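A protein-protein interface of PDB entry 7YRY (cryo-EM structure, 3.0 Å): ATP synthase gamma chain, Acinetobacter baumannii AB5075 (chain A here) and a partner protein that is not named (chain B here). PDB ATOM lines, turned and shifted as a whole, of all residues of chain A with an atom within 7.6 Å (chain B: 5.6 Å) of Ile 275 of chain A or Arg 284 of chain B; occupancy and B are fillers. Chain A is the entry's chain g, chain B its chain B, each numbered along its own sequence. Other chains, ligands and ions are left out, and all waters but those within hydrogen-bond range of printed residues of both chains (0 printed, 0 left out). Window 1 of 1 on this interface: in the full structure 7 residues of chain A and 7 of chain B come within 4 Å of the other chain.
Arg 284 of chain B touches Ile 275 of chain A.
Ile 279 of chain A touches Arg 284 of chain B (CD1 to CG, 3.8 Å).
Glu 285 of chain B touches Ile 282 of chain A.
Ile 282 of chain A touches Ala 286 of chain B (CD1 to N, 3.6 Å).
Ile 275 of chain A touches just one residue of chain B: Arg 284 (3.8 Å).
Printed residues of chain B within 4 Å of Ile 279 of chain A: Arg 284 (3.8 Å).
Of the printed residues of chain B, Ile 282 of chain A touches Glu 285 (3.8 Å) and Ala 286 (3.6 Å).
Of chain A, only Ile 275 and Ile 279 come within 4 Å of Arg 284 of chain B.
Of the printed residues of chain A, Ala 286 of chain B touches Ile 282 (3.6 Å).
The nearest printed residue of chain B that does not touch Ile 275 of chain A is Glu 285 of chain B (7.1 Å).
The nearest residue of chain A that does not touch Arg 284 of chain B is Ile 282 of chain A (5.0 Å).
Printed residues of chain A that touch a printed residue of chain B: Ile 275, Ile 279 and Ile 282.
Printed residues of chain B that touch a printed residue of chain A: Arg 284, Glu 285 and Ala 286.
Among the printed residues, 4 pairs touch across the chains.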
ATOM      1  N   ASN A 268     -17.720  19.390 -16.876  1.00  0.00           N
ATOM      2  CA  ASN A 268     -17.047  19.687 -18.138  1.00  0.00           C
ATOM      3  C   ASN A 268     -15.538  19.779 -17.948  1.00  0.00           C
ATOM      4  O   ASN A 268     -14.762  19.257 -18.767  1.00  0.00           O
ATOM      5  CB  ASN A 268     -17.597  20.982 -18.733  1.00  0.00           C
ATOM      6  CG  ASN A 268     -18.968  20.799 -19.346  1.00  0.00           C
ATOM      7  OD1 ASN A 268     -19.218  19.823 -20.053  1.00  0.00           O
ATOM      8  ND2 ASN A 268     -19.868  21.737 -19.078  1.00  0.00           N
ATOM      9  N   LYS A 269     -15.105  20.432 -16.864  1.00  0.00           N
ATOM     10  CA  LYS A 269     -13.673  20.508 -16.582  1.00  0.00           C
ATOM     11  C   LYS A 269     -13.065  19.113 -16.442  1.00  0.00           C
ATOM     12  O   LYS A 269     -12.020  18.807 -17.041  1.00  0.00           O
ATOM     13  CB  LYS A 269     -13.437  21.329 -15.315  1.00  0.00           C
ATOM     14  CG  LYS A 269     -11.976  21.557 -14.985  1.00  0.00           C
ATOM     15  CD  LYS A 269     -11.806  21.971 -13.535  1.00  0.00           C
ATOM     16  CE  LYS A 269     -11.441  23.439 -13.419  1.00  0.00           C
ATOM     17  NZ  LYS A 269      -9.982  23.622 -13.192  1.00  0.00           N
ATOM     18  N   LEU A 270     -13.725  18.246 -15.667  1.00  0.00           N
ATOM     19  CA  LEU A 270     -13.200  16.900 -15.456  1.00  0.00           C
ATOM     20  C   LEU A 270     -13.172  16.098 -16.752  1.00  0.00           C
ATOM     21  O   LEU A 270     -12.233  15.329 -16.993  1.00  0.00           O
ATOM     22  CB  LEU A 270     -14.023  16.170 -14.394  1.00  0.00           C
ATOM     23  CG  LEU A 270     -13.680  16.488 -12.939  1.00  0.00           C
ATOM     24  CD1 LEU A 270     -14.924  16.453 -12.073  1.00  0.00           C
ATOM     25  CD2 LEU A 270     -12.641  15.513 -12.417  1.00  0.00           C
ATOM     26  N   ARG A 271     -14.199  16.249 -17.593  1.00  0.00           N
ATOM     27  CA  ARG A 271     -14.237  15.517 -18.855  1.00  0.00           C
ATOM     28  C   ARG A 271     -13.076  15.916 -19.759  1.00  0.00           C
ATOM     29  O   ARG A 271     -12.410  15.057 -20.356  1.00  0.00           O
ATOM     30  CB  ARG A 271     -15.574  15.751 -19.558  1.00  0.00           C
ATOM     31  CG  ARG A 271     -15.564  15.438 -21.046  1.00  0.00           C
ATOM     32  CD  ARG A 271     -16.858  15.875 -21.712  1.00  0.00           C
ATOM     33  NE  ARG A 271     -16.835  17.285 -22.087  1.00  0.00           N
ATOM     34  CZ  ARG A 271     -16.227  17.766 -23.162  1.00  0.00           C
ATOM     35  NH1 ARG A 271     -15.587  16.975 -24.007  1.00  0.00           N
ATOM     36  NH2 ARG A 271     -16.259  19.075 -23.395  1.00  0.00           N
ATOM     37  N   GLN A 272     -12.815  17.223 -19.870  1.00  0.00           N
ATOM     38  CA  GLN A 272     -11.689  17.660 -20.690  1.00  0.00           C
ATOM     39  C   GLN A 272     -10.369  17.127 -20.141  1.00  0.00           C
ATOM     40  O   GLN A 272      -9.509  16.658 -20.904  1.00  0.00           O
ATOM     41  CB  GLN A 272     -11.657  19.185 -20.787  1.00  0.00           C
ATOM     42  CG  GLN A 272     -12.840  19.782 -21.526  1.00  0.00           C
ATOM     43  CD  GLN A 272     -12.713  21.280 -21.714  1.00  0.00           C
ATOM     44  OE1 GLN A 272     -11.625  21.796 -21.972  1.00  0.00           O
ATOM     45  NE2 GLN A 272     -13.827  21.989 -21.584  1.00  0.00           N
ATOM     46  N   ALA A 273     -10.199  17.177 -18.814  1.00  0.00           N
ATOM     47  CA  ALA A 273      -8.972  16.654 -18.218  1.00  0.00           C
ATOM     48  C   ALA A 273      -8.795  15.169 -18.522  1.00  0.00           C
ATOM     49  O   ALA A 273      -7.691  14.723 -18.860  1.00  0.00           O
ATOM     50  CB  ALA A 273      -8.979  16.895 -16.709  1.00  0.00           C
ATOM     51  N   ALA A 274      -9.876  14.393 -18.406  1.00  0.00           N
ATOM     52  CA  ALA A 274      -9.792  12.956 -18.656  1.00  0.00           C
ATOM     53  C   ALA A 274      -9.427  12.661 -20.104  1.00  0.00           C
ATOM     54  O   ALA A 274      -8.600  11.781 -20.376  1.00  0.00           O
ATOM     55  CB  ALA A 274     -11.114  12.283 -18.290  1.00  0.00           C
ATOM     56  N   ILE A 275     -10.038  13.380 -21.052  1.00  0.00           N
ATOM     57  CA  ILE A 275      -9.710  13.145 -22.457  1.00  0.00           C
ATOM     58  C   ILE A 275      -8.242  13.454 -22.718  1.00  0.00           C
ATOM     59  O   ILE A 275      -7.538  12.687 -23.396  1.00  0.00           O
ATOM     60  CB  ILE A 275     -10.631  13.962 -23.382  1.00  0.00           C
ATOM     61  CG1 ILE A 275     -12.094  13.599 -23.142  1.00  0.00           C
ATOM     62  CG2 ILE A 275     -10.275  13.697 -24.833  1.00  0.00           C
ATOM     63  CD1 ILE A 275     -13.064  14.475 -23.897  1.00  0.00           C
ATOM     64  N   THR A 276      -7.753  14.577 -22.179  1.00  0.00           N
ATOM     65  CA  THR A 276      -6.349  14.929 -22.379  1.00  0.00           C
ATOM     66  C   THR A 276      -5.422  13.868 -21.797  1.00  0.00           C
ATOM     67  O   THR A 276      -4.432  13.480 -22.432  1.00  0.00           O
ATOM     68  CB  THR A 276      -6.053  16.293 -21.754  1.00  0.00           C
ATOM     69  OG1 THR A 276      -7.013  17.251 -22.214  1.00  0.00           O
ATOM     70  CG2 THR A 276      -4.656  16.758 -22.132  1.00  0.00           C
ATOM     71  N   GLN A 277      -5.731  13.381 -20.591  1.00  0.00           N
ATOM     72  CA  GLN A 277      -4.872  12.386 -19.958  1.00  0.00           C
ATOM     73  C   GLN A 277      -4.848  11.089 -20.756  1.00  0.00           C
ATOM     74  O   GLN A 277      -3.782  10.496 -20.961  1.00  0.00           O
ATOM     75  CB  GLN A 277      -5.337  12.130 -18.523  1.00  0.00           C
ATOM     76  CG  GLN A 277      -5.025  10.737 -17.971  1.00  0.00           C
ATOM     77  CD  GLN A 277      -3.549  10.520 -17.662  1.00  0.00           C
ATOM     78  OE1 GLN A 277      -2.682  10.698 -18.516  1.00  0.00           O
ATOM     79  NE2 GLN A 277      -3.263  10.125 -16.428  1.00  0.00           N
ATOM     80  N   GLU A 278      -6.015  10.635 -21.225  1.00  0.00           N
ATOM     81  CA  GLU A 278      -6.056   9.404 -22.011  1.00  0.00           C
ATOM     82  C   GLU A 278      -5.276   9.544 -23.313  1.00  0.00           C
ATOM     83  O   GLU A 278      -4.544   8.625 -23.709  1.00  0.00           O
ATOM     84  CB  GLU A 278      -7.503   9.000 -22.284  1.00  0.00           C
ATOM     85  CG  GLU A 278      -8.010   7.855 -21.411  1.00  0.00           C
ATOM     86  CD  GLU A 278      -7.852   8.113 -19.924  1.00  0.00           C
ATOM     87  OE1 GLU A 278      -7.531   7.157 -19.188  1.00  0.00           O
ATOM     88  OE2 GLU A 278      -8.059   9.263 -19.485  1.00  0.00           O
ATOM     89  N   ILE A 279      -5.411  10.684 -23.995  1.00  0.00           N
ATOM     90  CA  ILE A 279      -4.683  10.873 -25.248  1.00  0.00           C
ATOM     91  C   ILE A 279      -3.179  10.892 -24.995  1.00  0.00           C
ATOM     92  O   ILE A 279      -2.399  10.280 -25.742  1.00  0.00           O
ATOM     93  CB  ILE A 279      -5.166  12.150 -25.960  1.00  0.00           C
ATOM     94  CG1 ILE A 279      -6.387  11.828 -26.820  1.00  0.00           C
ATOM     95  CG2 ILE A 279      -4.062  12.742 -26.819  1.00  0.00           C
ATOM     96  CD1 ILE A 279      -7.373  12.955 -26.922  1.00  0.00           C
ATOM     97  N   SER A 280      -2.747  11.584 -23.936  1.00  0.00           N
ATOM     98  CA  SER A 280      -1.325  11.614 -23.612  1.00  0.00           C
ATOM     99  C   SER A 280      -0.802  10.221 -23.288  1.00  0.00           C
ATOM    100  O   SER A 280       0.302   9.852 -23.708  1.00  0.00           O
ATOM    101  CB  SER A 280      -1.072  12.564 -22.442  1.00  0.00           C
ATOM    102  OG  SER A 280       0.229  12.374 -21.914  1.00  0.00           O
ATOM    103  N   GLU A 281      -1.576   9.435 -22.537  1.00  0.00           N
ATOM    104  CA  GLU A 281      -1.153   8.078 -22.205  1.00  0.00           C
ATOM    105  C   GLU A 281      -1.024   7.219 -23.458  1.00  0.00           C
ATOM    106  O   GLU A 281      -0.055   6.463 -23.604  1.00  0.00           O
ATOM    107  CB  GLU A 281      -2.141   7.444 -21.227  1.00  0.00           C
ATOM    108  CG  GLU A 281      -2.177   5.926 -21.284  1.00  0.00           C
ATOM    109  CD  GLU A 281      -3.561   5.365 -21.041  1.00  0.00           C
ATOM    110  OE1 GLU A 281      -4.041   5.444 -19.891  1.00  0.00           O
ATOM    111  OE2 GLU A 281      -4.167   4.839 -21.997  1.00  0.00           O
ATOM    112  N   ILE A 282      -1.988   7.328 -24.375  1.00  0.00           N
ATOM    113  CA  ILE A 282      -1.937   6.535 -25.600  1.00  0.00           C
ATOM    114  C   ILE A 282      -0.718   6.917 -26.431  1.00  0.00           C
ATOM    115  O   ILE A 282      -0.006   6.048 -26.955  1.00  0.00           O
ATOM    116  CB  ILE A 282      -3.244   6.695 -26.397  1.00  0.00           C
ATOM    117  CG1 ILE A 282      -4.321   5.762 -25.839  1.00  0.00           C
ATOM    118  CG2 ILE A 282      -3.015   6.417 -27.875  1.00  0.00           C
ATOM    119  CD1 ILE A 282      -5.709   6.057 -26.356  1.00  0.00           C
ATOM    120  N   PRO B 282      -2.312   6.635 -34.033  1.00  0.00           N
ATOM    121  CA  PRO B 282      -3.622   6.648 -33.374  1.00  0.00           C
ATOM    122  C   PRO B 282      -4.075   8.058 -33.022  1.00  0.00           C
ATOM    123  O   PRO B 282      -3.280   8.993 -32.901  1.00  0.00           O
ATOM    124  CB  PRO B 282      -3.390   5.815 -32.109  1.00  0.00           C
ATOM    125  CG  PRO B 282      -1.929   5.943 -31.843  1.00  0.00           C
ATOM    126  CD  PRO B 282      -1.268   6.032 -33.186  1.00  0.00           C
ATOM    127  N   GLY B 283      -5.387   8.195 -32.859  1.00  0.00           N
ATOM    128  CA  GLY B 283      -5.986   9.431 -32.391  1.00  0.00           C
ATOM    129  C   GLY B 283      -6.637   9.250 -31.036  1.00  0.00           C
ATOM    130  O   GLY B 283      -6.069   8.595 -30.158  1.00  0.00           O
ATOM    131  N   ARG B 284      -7.818   9.833 -30.842  1.00  0.00           N
ATOM    132  CA  ARG B 284      -8.559   9.603 -29.609  1.00  0.00           C
ATOM    133  C   ARG B 284      -8.969   8.140 -29.499  1.00  0.00           C
ATOM    134  O   ARG B 284      -9.493   7.558 -30.453  1.00  0.00           O
ATOM    135  CB  ARG B 284      -9.797  10.497 -29.549  1.00  0.00           C
ATOM    136  CG  ARG B 284      -9.551  11.953 -29.889  1.00  0.00           C
ATOM    137  CD  ARG B 284     -10.862  12.719 -30.040  1.00  0.00           C
ATOM    138  NE  ARG B 284     -11.549  12.917 -28.768  1.00  0.00           N
ATOM    139  CZ  ARG B 284     -12.490  12.117 -28.288  1.00  0.00           C
ATOM    140  NH1 ARG B 284     -12.901  11.052 -28.958  1.00  0.00           N
ATOM    141  NH2 ARG B 284     -13.037  12.393 -27.107  1.00  0.00           N
ATOM    142  N   GLU B 285      -8.726   7.552 -28.326  1.00  0.00           N
ATOM    143  CA  GLU B 285      -9.094   6.164 -28.034  1.00  0.00           C
ATOM    144  C   GLU B 285      -8.487   5.191 -29.041  1.00  0.00           C
ATOM    145  O   GLU B 285      -9.087   4.162 -29.361  1.00  0.00           O
ATOM    146  CB  GLU B 285     -10.614   5.992 -27.977  1.00  0.00           C
ATOM    147  CG  GLU B 285     -11.301   6.933 -27.010  1.00  0.00           C
ATOM    148  CD  GLU B 285     -12.788   7.031 -27.261  1.00  0.00           C
ATOM    149  OE1 GLU B 285     -13.225   6.696 -28.382  1.00  0.00           O
ATOM    150  OE2 GLU B 285     -13.521   7.445 -26.339  1.00  0.00           O
ATOM    151  N   ALA B 286      -7.302   5.524 -29.552  1.00  0.00           N
ATOM    152  CA  ALA B 286      -6.537   4.749 -30.523  1.00  0.00           C
ATOM    153  C   ALA B 286      -7.238   4.616 -31.870  1.00  0.00           C
ATOM    154  O   ALA B 286      -6.735   3.899 -32.743  1.00  0.00           O
ATOM    155  CB  ALA B 286      -6.184   3.347 -30.006  1.00  0.00           C
ATOM    156  N   TYR B 287      -8.379   5.269 -32.069  1.00  0.00           N
ATOM    157  CA  TYR B 287      -9.004   5.276 -33.382  1.00  0.00           C
ATOM    158  C   TYR B 287      -8.113   6.011 -34.380  1.00  0.00           C
ATOM    159  O   TYR B 287      -7.483   7.015 -34.028  1.00  0.00           O
ATOM    160  CB  TYR B 287     -10.379   5.943 -33.331  1.00  0.00           C
ATOM    161  CG  TYR B 287     -11.455   5.121 -32.665  1.00  0.00           C
ATOM    162  CD1 TYR B 287     -11.714   3.822 -33.074  1.00  0.00           C
ATOM    163  CD2 TYR B 287     -12.224   5.652 -31.641  1.00  0.00           C
ATOM    164  CE1 TYR B 287     -12.701   3.069 -32.473  1.00  0.00           C
ATOM    165  CE2 TYR B 287     -13.214   4.906 -31.034  1.00  0.00           C
ATOM    166  CZ  TYR B 287     -13.449   3.616 -31.454  1.00  0.00           C
ATOM    167  OH  TYR B 287     -14.436   2.873 -30.850  1.00  0.00           O
ATOM    168  N   PHE B 341     -17.358   9.048 -28.900  1.00  0.00           N
ATOM    169  CA  PHE B 341     -16.791   9.441 -30.186  1.00  0.00           C
ATOM    170  C   PHE B 341     -17.608   8.896 -31.355  1.00  0.00           C
ATOM    171  O   PHE B 341     -18.183   9.661 -32.143  1.00  0.00           O
ATOM    172  CB  PHE B 341     -15.341   8.961 -30.263  1.00  0.00           C
ATOM    173  CG  PHE B 341     -14.560   9.570 -31.386  1.00  0.00           C
ATOM    174  CD1 PHE B 341     -14.874  10.829 -31.862  1.00  0.00           C
ATOM    175  CD2 PHE B 341     -13.507   8.882 -31.962  1.00  0.00           C
ATOM    176  CE1 PHE B 341     -14.155  11.391 -32.895  1.00  0.00           C
ATOM    177  CE2 PHE B 341     -12.782   9.438 -32.996  1.00  0.00           C
ATOM    178  CZ  PHE B 341     -13.108  10.695 -33.463  1.00  0.00           C
